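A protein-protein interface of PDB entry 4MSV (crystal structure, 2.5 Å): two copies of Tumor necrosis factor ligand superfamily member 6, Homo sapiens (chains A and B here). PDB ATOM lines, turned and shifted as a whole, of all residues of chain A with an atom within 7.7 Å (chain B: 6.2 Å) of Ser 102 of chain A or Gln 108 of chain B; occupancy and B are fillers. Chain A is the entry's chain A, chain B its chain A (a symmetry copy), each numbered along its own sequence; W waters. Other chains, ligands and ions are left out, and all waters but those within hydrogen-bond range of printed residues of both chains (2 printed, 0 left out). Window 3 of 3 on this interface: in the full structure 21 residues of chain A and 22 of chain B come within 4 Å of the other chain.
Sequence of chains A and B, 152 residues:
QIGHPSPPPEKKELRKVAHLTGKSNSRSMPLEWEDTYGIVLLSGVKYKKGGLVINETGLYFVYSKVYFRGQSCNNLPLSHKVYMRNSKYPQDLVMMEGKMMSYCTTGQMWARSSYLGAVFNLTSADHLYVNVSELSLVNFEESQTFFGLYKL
The guanidinium group of Arg 112 of chain B lies within hydrogen-bond range of the backbone carbonyl oxygen of Met 101 of chain A (2.8 Å).
The backbone carbonyl oxygen of Ser 102 of chain A lies close to the backbone carbonyl oxygen of Tyr 103 of chain B (3.1 Å).
The backbone NH of Thr 105 of chain B lies within hydrogen-bond range of the side-chain hydroxyl of Ser 102 of chain A (2.9 Å).
O of Ser 102 of chain A lies within hydrogen-bond range of NH2 of Arg 112 of chain B, at 2.8 Å.
O of Met 101 of chain A is in hydrogen-bond range of N of Ala 111 of chain B.
N of Cys 73 of chain B lies within hydrogen-bond range of O of Gln 108 of chain B.
The backbone carbonyl oxygen (O) of Tyr 103 of chain A sits at hydrogen-bond distance from the guanidinium group (NH1) of Arg 112 of chain A (3.0 Å).
The backbone carbonyl oxygen of Gly 70 of chain B lies within hydrogen-bond range of the backbone NH of Trp 110 of chain B (2.9 Å).
SG of Cys 104 of chain A is disulfide-bonded to SG of Cys 73 of chain A.
The side-chain amide nitrogen (ND2) of Asn 75 of chain A is in hydrogen-bond range of the backbone carbonyl oxygen (O) of Cys 104 of chain A.
The side-chain hydroxyl of Tyr 103 of chain A lies within hydrogen-bond range of the backbone carbonyl oxygen of Leu 76 of chain A, 2.5 Å away.
Among the printed residues, pairs that only touch across the chains: Ser 102 of chain A with Met 109 of chain B (3.3 Å), Ser 102 of chain A with Cys 104 of chain B (3.3 Å), Met 101 of chain A with Trp 110 of chain B (3.4 Å), Met 100 of chain A with Ala 111 of chain B (3.4 Å), Tyr 103 of chain A with Arg 112 of chain B (3.6 Å), Ser 102 of chain A with Gln 108 of chain B (3.7 Å), Cys 104 of chain A with Thr 105 of chain B (3.8 Å), Met 101 of chain A with Met 109 of chain B (3.8 Å) and Ser 102 of chain A with Trp 110 of chain B (3.9 Å).
Of chain B, only Tyr 103 (3.1 Å), Cys 104 (3.3 Å), Thr 105 (2.9 Å), Gln 108 (3.7 Å), Met 109 (3.3 Å), Trp 110 (3.9 Å) and Arg 112 (2.8 Å) come within 4 Å of Ser 102 of chain A.
Gln 108 of chain B touches just one residue of chain A: Ser 102.
No residue of chain A comes within 4 Å of Gly 107 of chain B.
Of the printed residues of chain A, Cys 104 of chain B touches Ser 102.
Of the printed residues of chain A, Met 109 of chain B touches Met 101 (3.8 Å) and Ser 102 (3.3 Å).
Arg 112 of chain A touches none of the printed residues of chain B.
Thr 106 of chain A touches none of the printed residues of chain B.
The nearest residue of chain B that does not touch Ser 102 of chain A is Ala 111 of chain B (5.0 Å).
Of the 14 printed residues of chain A, 5 touch a printed residue of chain B.
Of the 14 printed residues of chain B, 8 touch a printed residue of chain A.
Printed residues of chain B that touch a printed residue of chain A: Tyr 103, Cys 104, Thr 105, Gln 108, Met 109, Trp 110, Ala 111 and Arg 112.
Among the printed residues, 14 pairs touch across the chains.
Among the printed residues, no Asp or Glu carboxylate lies within 4 Å of a Lys or Arg side-chain nitrogen of the other chain.
Tyr 103 of chain A touches Arg 112 of chain B, but with the chains exchanged Arg 112 of chain A does not touch Tyr 103 of chain B (5.9 Å).
Cys 104 of chain A touches Thr 105 of chain B, but with the chains exchanged Thr 105 of chain A does not touch Cys 104 of chain B (7.2 Å).
Positions printed for both chains: 73, 103, 104, 105, 106 and 112.
Of the 14 pairs that touch across the chains among the printed residues, none has its exchanged pair printed and touching as well.
Water W1 lies within hydrogen-bond range of OG1 of Thr 105 of chain B, O of Cys 104 of chain A and O of Ser 102 of chain A.
Water W2 lies within hydrogen-bond range of N of Thr 106 of chain A (2.7 Å) and OG1 of Thr 105 of chain B (3.0 Å).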
ATOM      1  N   CYS A  73      -9.820 -14.231  -2.115  1.00  0.00           N
ATOM      2  CA  CYS A  73      -9.206 -13.113  -2.810  1.00  0.00           C
ATOM      3  C   CYS A  73      -8.560 -13.513  -4.132  1.00  0.00           C
ATOM      4  O   CYS A  73      -7.762 -14.440  -4.134  1.00  0.00           O
ATOM      5  CB  CYS A  73      -8.093 -12.578  -1.924  1.00  0.00           C
ATOM      6  SG  CYS A  73      -7.114 -11.187  -2.534  1.00  0.00           S
ATOM      7  N   ASN A  74      -8.871 -12.796  -5.218  1.00  0.00           N
ATOM      8  CA  ASN A  74      -8.031 -12.770  -6.428  1.00  0.00           C
ATOM      9  C   ASN A  74      -7.629 -11.350  -6.844  1.00  0.00           C
ATOM     10  O   ASN A  74      -7.230 -11.134  -8.005  1.00  0.00           O
ATOM     11  CB  ASN A  74      -8.670 -13.478  -7.626  1.00  0.00           C
ATOM     12  CG  ASN A  74     -10.116 -13.068  -7.870  1.00  0.00           C
ATOM     13  OD1 ASN A  74     -10.586 -11.936  -7.631  1.00  0.00           O
ATOM     14  ND2 ASN A  74     -10.848 -14.025  -8.367  1.00  0.00           N
ATOM     15  N   ASN A  75      -7.726 -10.400  -5.916  1.00  0.00           N
ATOM     16  CA  ASN A  75      -7.307  -9.058  -6.195  1.00  0.00           C
ATOM     17  C   ASN A  75      -7.844  -8.436  -7.504  1.00  0.00           C
ATOM     18  O   ASN A  75      -7.142  -7.730  -8.233  1.00  0.00           O
ATOM     19  CB  ASN A  75      -5.781  -9.009  -6.155  1.00  0.00           C
ATOM     20  CG  ASN A  75      -5.246  -9.017  -4.732  1.00  0.00           C
ATOM     21  OD1 ASN A  75      -5.443  -8.063  -3.956  1.00  0.00           O
ATOM     22  ND2 ASN A  75      -4.574 -10.085  -4.366  1.00  0.00           N
ATOM     23  N   LEU A  76      -9.075  -8.723  -7.806  1.00  0.00           N
ATOM     24  CA  LEU A  76      -9.854  -7.973  -8.800  1.00  0.00           C
ATOM     25  C   LEU A  76      -9.904  -6.503  -8.406  1.00  0.00           C
ATOM     26  O   LEU A  76     -10.242  -6.183  -7.288  1.00  0.00           O
ATOM     27  CB  LEU A  76     -11.294  -8.471  -8.783  1.00  0.00           C
ATOM     28  CG  LEU A  76     -11.926  -8.970 -10.066  1.00  0.00           C
ATOM     29  CD1 LEU A  76     -10.906  -9.769 -10.880  1.00  0.00           C
ATOM     30  CD2 LEU A  76     -13.180  -9.798  -9.726  1.00  0.00           C
ATOM     31  N   PRO A  77      -9.581  -5.612  -9.333  1.00  0.00           N
ATOM     32  CA  PRO A  77      -9.563  -4.200  -8.956  1.00  0.00           C
ATOM     33  C   PRO A  77     -10.905  -3.732  -8.554  1.00  0.00           C
ATOM     34  O   PRO A  77     -11.889  -4.077  -9.181  1.00  0.00           O
ATOM     35  CB  PRO A  77      -9.142  -3.468 -10.266  1.00  0.00           C
ATOM     36  CG  PRO A  77      -8.317  -4.517 -11.015  1.00  0.00           C
ATOM     37  CD  PRO A  77      -8.820  -5.882 -10.574  1.00  0.00           C
ATOM     38  N   LEU A  78     -10.961  -2.973  -7.493  1.00  0.00           N
ATOM     39  CA  LEU A  78     -12.215  -2.478  -7.017  1.00  0.00           C
ATOM     40  C   LEU A  78     -12.182  -1.017  -7.173  1.00  0.00           C
ATOM     41  O   LEU A  78     -11.203  -0.394  -6.847  1.00  0.00           O
ATOM     42  CB  LEU A  78     -12.382  -2.753  -5.561  1.00  0.00           C
ATOM     43  CG  LEU A  78     -12.262  -4.213  -5.084  1.00  0.00           C
ATOM     44  CD1 LEU A  78     -12.171  -4.238  -3.554  1.00  0.00           C
ATOM     45  CD2 LEU A  78     -13.451  -5.046  -5.564  1.00  0.00           C
ATOM     46  N   MET A 100      -9.039   0.312  -5.445  1.00  0.00           N
ATOM     47  CA  MET A 100      -8.160  -0.564  -4.663  1.00  0.00           C
ATOM     48  C   MET A 100      -7.589  -1.649  -5.546  1.00  0.00           C
ATOM     49  O   MET A 100      -8.336  -2.285  -6.223  1.00  0.00           O
ATOM     50  CB  MET A 100      -8.881  -1.245  -3.527  1.00  0.00           C
ATOM     51  CG  MET A 100      -9.534  -0.235  -2.606  1.00  0.00           C
ATOM     52  SD  MET A 100     -10.192  -1.169  -1.203  1.00  0.00           S
ATOM     53  CE  MET A 100     -11.596  -0.159  -0.850  1.00  0.00           C
ATOM     54  N   MET A 101      -6.267  -1.819  -5.507  1.00  0.00           N
ATOM     55  CA  MET A 101      -5.593  -2.909  -6.165  1.00  0.00           C
ATOM     56  C   MET A 101      -4.502  -3.438  -5.242  1.00  0.00           C
ATOM     57  O   MET A 101      -3.885  -2.687  -4.504  1.00  0.00           O
ATOM     58  CB  MET A 101      -5.001  -2.502  -7.500  1.00  0.00           C
ATOM     59  CG  MET A 101      -5.985  -2.019  -8.589  1.00  0.00           C
ATOM     60  SD  MET A 101      -5.166  -1.509 -10.165  1.00  0.00           S
ATOM     61  CE  MET A 101      -4.240  -2.971 -10.505  1.00  0.00           C
ATOM     62  N   SER A 102      -4.349  -4.757  -5.252  1.00  0.00           N
ATOM     63  CA  SER A 102      -3.446  -5.497  -4.384  1.00  0.00           C
ATOM     64  C   SER A 102      -3.791  -5.236  -2.946  1.00  0.00           C
ATOM     65  O   SER A 102      -2.950  -4.849  -2.144  1.00  0.00           O
ATOM     66  CB  SER A 102      -1.964  -5.198  -4.661  1.00  0.00           C
ATOM     67  OG  SER A 102      -1.121  -6.210  -4.040  1.00  0.00           O
ATOM     68  N   TYR A 103      -5.044  -5.486  -2.632  1.00  0.00           N
ATOM     69  CA  TYR A 103      -5.575  -5.243  -1.302  1.00  0.00           C
ATOM     70  C   TYR A 103      -5.717  -6.526  -0.442  1.00  0.00           C
ATOM     71  O   TYR A 103      -6.079  -6.462   0.724  1.00  0.00           O
ATOM     72  CB  TYR A 103      -6.927  -4.482  -1.395  1.00  0.00           C
ATOM     73  CG  TYR A 103      -7.898  -5.133  -2.313  1.00  0.00           C
ATOM     74  CD1 TYR A 103      -7.910  -4.842  -3.662  1.00  0.00           C
ATOM     75  CD2 TYR A 103      -8.718  -6.091  -1.875  1.00  0.00           C
ATOM     76  CE1 TYR A 103      -8.739  -5.497  -4.547  1.00  0.00           C
ATOM     77  CE2 TYR A 103      -9.576  -6.793  -2.762  1.00  0.00           C
ATOM     78  CZ  TYR A 103      -9.578  -6.492  -4.099  1.00  0.00           C
ATOM     79  OH  TYR A 103     -10.440  -7.145  -4.960  1.00  0.00           O
ATOM     80  N   CYS A 104      -5.520  -7.702  -0.980  1.00  0.00           N
ATOM     81  CA  CYS A 104      -5.616  -8.890  -0.079  1.00  0.00           C
ATOM     82  C   CYS A 104      -4.666  -9.933  -0.486  1.00  0.00           C
ATOM     83  O   CYS A 104      -4.024  -9.791  -1.529  1.00  0.00           O
ATOM     84  CB  CYS A 104      -7.031  -9.478  -0.009  1.00  0.00           C
ATOM     85  SG  CYS A 104      -7.886  -9.570  -1.617  1.00  0.00           S
ATOM     86  N   THR A 105      -4.532 -10.948   0.361  1.00  0.00           N
ATOM     87  CA  THR A 105      -3.573 -12.005   0.118  1.00  0.00           C
ATOM     88  C   THR A 105      -4.309 -13.076  -0.679  1.00  0.00           C
ATOM     89  O   THR A 105      -5.371 -13.513  -0.263  1.00  0.00           O
ATOM     90  CB  THR A 105      -3.038 -12.589   1.437  1.00  0.00           C
ATOM     91  OG1 THR A 105      -2.167 -11.652   2.078  1.00  0.00           O
ATOM     92  CG2 THR A 105      -2.273 -13.919   1.163  1.00  0.00           C
ATOM     93  N   THR A 106      -3.763 -13.476  -1.825  1.00  0.00           N
ATOM     94  CA  THR A 106      -4.448 -14.411  -2.697  1.00  0.00           C
ATOM     95  C   THR A 106      -5.011 -15.639  -2.023  1.00  0.00           C
ATOM     96  O   THR A 106      -4.314 -16.282  -1.298  1.00  0.00           O
ATOM     97  CB  THR A 106      -3.497 -14.886  -3.739  1.00  0.00           C
ATOM     98  OG1 THR A 106      -3.128 -13.735  -4.498  1.00  0.00           O
ATOM     99  CG2 THR A 106      -4.197 -15.944  -4.644  1.00  0.00           C
ATOM    100  N   ARG A 112     -12.970  -5.096   2.820  1.00  0.00           N
ATOM    101  CA  ARG A 112     -12.419  -3.736   2.890  1.00  0.00           C
ATOM    102  C   ARG A 112     -13.507  -2.792   2.452  1.00  0.00           C
ATOM    103  O   ARG A 112     -14.343  -3.156   1.614  1.00  0.00           O
ATOM    104  CB  ARG A 112     -11.190  -3.583   1.981  1.00  0.00           C
ATOM    105  CG  ARG A 112     -10.083  -2.533   2.511  1.00  0.00           C
ATOM    106  CD  ARG A 112      -9.327  -3.004   3.781  1.00  0.00           C
ATOM    107  NE  ARG A 112      -9.124  -4.456   3.688  1.00  0.00           N
ATOM    108  CZ  ARG A 112      -8.173  -5.075   3.043  1.00  0.00           C
ATOM    109  NH1 ARG A 112      -7.274  -4.386   2.472  1.00  0.00           N
ATOM    110  NH2 ARG A 112      -8.141  -6.427   2.961  1.00  0.00           N
ATOM    111  N   GLY B  70       1.143   2.490  -7.492  1.00  0.00           N
ATOM    112  CA  GLY B  70       2.488   2.148  -7.973  1.00  0.00           C
ATOM    113  C   GLY B  70       2.470   0.835  -8.762  1.00  0.00           C
ATOM    114  O   GLY B  70       1.616  -0.037  -8.502  1.00  0.00           O
ATOM    115  N   GLN B  71       3.385   0.713  -9.729  1.00  0.00           N
ATOM    116  CA  GLN B  71       3.570  -0.472 -10.589  1.00  0.00           C
ATOM    117  C   GLN B  71       3.965  -1.704  -9.818  1.00  0.00           C
ATOM    118  O   GLN B  71       3.577  -2.805 -10.189  1.00  0.00           O
ATOM    119  CB  GLN B  71       4.744  -0.261 -11.585  1.00  0.00           C
ATOM    120  CG  GLN B  71       4.291   0.273 -12.869  1.00  0.00           C
ATOM    121  CD  GLN B  71       4.615   1.734 -13.011  1.00  0.00           C
ATOM    122  OE1 GLN B  71       4.478   2.547 -12.077  1.00  0.00           O
ATOM    123  NE2 GLN B  71       5.007   2.092 -14.211  1.00  0.00           N
ATOM    124  N   SER B  72       4.813  -1.523  -8.820  1.00  0.00           N
ATOM    125  CA  SER B  72       5.464  -2.628  -8.212  1.00  0.00           C
ATOM    126  C   SER B  72       5.589  -2.349  -6.715  1.00  0.00           C
ATOM    127  O   SER B  72       6.429  -1.607  -6.264  1.00  0.00           O
ATOM    128  CB  SER B  72       6.832  -2.809  -8.889  1.00  0.00           C
ATOM    129  OG  SER B  72       7.407  -3.981  -8.417  1.00  0.00           O
ATOM    130  N   CYS B  73       4.692  -2.931  -5.952  1.00  0.00           N
ATOM    131  CA  CYS B  73       4.685  -2.744  -4.511  1.00  0.00           C
ATOM    132  C   CYS B  73       6.014  -3.103  -3.856  1.00  0.00           C
ATOM    133  O   CYS B  73       6.502  -4.199  -4.090  1.00  0.00           O
ATOM    134  CB  CYS B  73       3.644  -3.688  -3.932  1.00  0.00           C
ATOM    135  SG  CYS B  73       3.417  -3.708  -2.140  1.00  0.00           S
ATOM    136  N   TYR B 103       0.464  -2.826   3.085  1.00  0.00           N
ATOM    137  CA  TYR B 103      -0.789  -2.639   2.375  1.00  0.00           C
ATOM    138  C   TYR B 103      -0.837  -3.346   0.995  1.00  0.00           C
ATOM    139  O   TYR B 103      -1.857  -3.337   0.321  1.00  0.00           O
ATOM    140  CB  TYR B 103      -1.105  -1.124   2.236  1.00  0.00           C
ATOM    141  CG  TYR B 103       0.023  -0.344   1.665  1.00  0.00           C
ATOM    142  CD1 TYR B 103       1.013   0.176   2.475  1.00  0.00           C
ATOM    143  CD2 TYR B 103       0.165  -0.211   0.345  1.00  0.00           C
ATOM    144  CE1 TYR B 103       2.115   0.825   1.961  1.00  0.00           C
ATOM    145  CE2 TYR B 103       1.296   0.441  -0.217  1.00  0.00           C
ATOM    146  CZ  TYR B 103       2.269   0.954   0.599  1.00  0.00           C
ATOM    147  OH  TYR B 103       3.351   1.625   0.060  1.00  0.00           O
ATOM    148  N   CYS B 104       0.242  -3.898   0.503  1.00  0.00           N
ATOM    149  CA  CYS B 104       0.108  -4.612  -0.803  1.00  0.00           C
ATOM    150  C   CYS B 104       1.002  -5.776  -0.855  1.00  0.00           C
ATOM    151  O   CYS B 104       1.806  -5.962   0.059  1.00  0.00           O
ATOM    152  CB  CYS B 104       0.369  -3.705  -2.012  1.00  0.00           C
ATOM    153  SG  CYS B 104       1.786  -2.574  -1.812  1.00  0.00           S
ATOM    154  N   THR B 105       0.821  -6.590  -1.891  1.00  0.00           N
ATOM    155  CA  THR B 105       1.582  -7.815  -2.023  1.00  0.00           C
ATOM    156  C   THR B 105       2.829  -7.459  -2.824  1.00  0.00           C
ATOM    157  O   THR B 105       2.715  -6.878  -3.892  1.00  0.00           O
ATOM    158  CB  THR B 105       0.770  -8.902  -2.749  1.00  0.00           C
ATOM    159  OG1 THR B 105      -0.276  -9.389  -1.902  1.00  0.00           O
ATOM    160  CG2 THR B 105       1.703 -10.079  -3.165  1.00  0.00           C
ATOM    161  N   THR B 106       4.009  -7.783  -2.301  1.00  0.00           N
ATOM    162  CA  THR B 106       5.249  -7.387  -2.942  1.00  0.00           C
ATOM    163  C   THR B 106       5.332  -7.661  -4.424  1.00  0.00           C
ATOM    164  O   THR B 106       5.055  -8.745  -4.837  1.00  0.00           O
ATOM    165  CB  THR B 106       6.379  -8.116  -2.303  1.00  0.00           C
ATOM    166  OG1 THR B 106       6.409  -7.690  -0.941  1.00  0.00           O
ATOM    167  CG2 THR B 106       7.711  -7.754  -3.025  1.00  0.00           C
ATOM    168  N   GLY B 107       5.696  -6.651  -5.206  1.00  0.00           N
ATOM    169  CA  GLY B 107       5.852  -6.783  -6.655  1.00  0.00           C
ATOM    170  C   GLY B 107       4.617  -6.545  -7.516  1.00  0.00           C
ATOM    171  O   GLY B 107       4.752  -6.415  -8.705  1.00  0.00           O
ATOM    172  N   GLN B 108       3.416  -6.464  -6.939  1.00  0.00           N
ATOM    173  CA  GLN B 108       2.201  -6.217  -7.728  1.00  0.00           C
ATOM    174  C   GLN B 108       1.877  -4.754  -8.006  1.00  0.00           C
ATOM    175  O   GLN B 108       2.310  -3.874  -7.298  1.00  0.00           O
ATOM    176  CB  GLN B 108       0.982  -6.843  -6.991  1.00  0.00           C
ATOM    177  CG  GLN B 108       1.142  -8.344  -6.735  1.00  0.00           C
ATOM    178  CD  GLN B 108       1.349  -9.070  -8.058  1.00  0.00           C
ATOM    179  OE1 GLN B 108       2.399  -9.564  -8.330  1.00  0.00           O
ATOM    180  NE2 GLN B 108       0.350  -9.060  -8.901  1.00  0.00           N
ATOM    181  N   MET B 109       1.085  -4.490  -9.048  1.00  0.00           N
ATOM    182  CA  MET B 109       0.472  -3.199  -9.201  1.00  0.00           C
ATOM    183  C   MET B 109      -0.475  -2.963  -8.014  1.00  0.00           C
ATOM    184  O   MET B 109      -1.175  -3.854  -7.609  1.00  0.00           O
ATOM    185  CB  MET B 109      -0.396  -3.142 -10.455  1.00  0.00           C
ATOM    186  CG  MET B 109       0.349  -3.142 -11.787  1.00  0.00           C
ATOM    187  SD  MET B 109      -0.761  -3.422 -13.209  1.00  0.00           S
ATOM    188  CE  MET B 109      -1.058  -5.201 -12.968  1.00  0.00           C
ATOM    189  N   TRP B 110      -0.524  -1.756  -7.485  1.00  0.00           N
ATOM    190  CA  TRP B 110      -1.281  -1.505  -6.295  1.00  0.00           C
ATOM    191  C   TRP B 110      -1.875  -0.127  -6.322  1.00  0.00           C
ATOM    192  O   TRP B 110      -1.395   0.770  -7.025  1.00  0.00           O
ATOM    193  CB  TRP B 110      -0.395  -1.696  -5.059  1.00  0.00           C
ATOM    194  CG  TRP B 110       0.706  -0.734  -4.924  1.00  0.00           C
ATOM    195  CD1 TRP B 110       1.916  -0.862  -5.424  1.00  0.00           C
ATOM    196  CD2 TRP B 110       0.688   0.507  -4.210  1.00  0.00           C
ATOM    197  NE1 TRP B 110       2.689   0.226  -5.109  1.00  0.00           N
ATOM    198  CE2 TRP B 110       1.956   1.079  -4.349  1.00  0.00           C
ATOM    199  CE3 TRP B 110      -0.294   1.208  -3.512  1.00  0.00           C
ATOM    200  CZ2 TRP B 110       2.274   2.303  -3.846  1.00  0.00           C
ATOM    201  CZ3 TRP B 110       0.016   2.425  -3.005  1.00  0.00           C
ATOM    202  CH2 TRP B 110       1.296   2.972  -3.173  1.00  0.00           C
ATOM    203  N   ALA B 111      -2.924   0.040  -5.520  1.00  0.00           N
ATOM    204  CA  ALA B 111      -3.540   1.347  -5.329  1.00  0.00           C
ATOM    205  C   ALA B 111      -4.351   1.376  -4.036  1.00  0.00           C
ATOM    206  O   ALA B 111      -5.045   0.374  -3.689  1.00  0.00           O
ATOM    207  CB  ALA B 111      -4.443   1.637  -6.496  1.00  0.00           C
ATOM    208  N   ARG B 112      -4.316   2.522  -3.337  1.00  0.00           N
ATOM    209  CA  ARG B 112      -5.101   2.658  -2.102  1.00  0.00           C
ATOM    210  C   ARG B 112      -5.223   4.129  -1.812  1.00  0.00           C
ATOM    211  O   ARG B 112      -4.315   4.903  -2.142  1.00  0.00           O
ATOM    212  CB  ARG B 112      -4.419   1.943  -0.925  1.00  0.00           C
ATOM    213  CG  ARG B 112      -5.432   1.340   0.178  1.00  0.00           C
ATOM    214  CD  ARG B 112      -6.262   0.131  -0.325  1.00  0.00           C
ATOM    215  NE  ARG B 112      -5.416  -0.677  -1.212  1.00  0.00           N
ATOM    216  CZ  ARG B 112      -4.546  -1.584  -0.854  1.00  0.00           C
ATOM    217  NH1 ARG B 112      -4.433  -1.868   0.377  1.00  0.00           N
ATOM    218  NH2 ARG B 112      -3.759  -2.205  -1.766  1.00  0.00           N
HETATM  219  O   HOH W   1      -1.837  -7.680  -1.247  1.00  0.00           O
HETATM  220  O   HOH W   2      -1.460 -12.124  -2.438  1.00  0.00           O
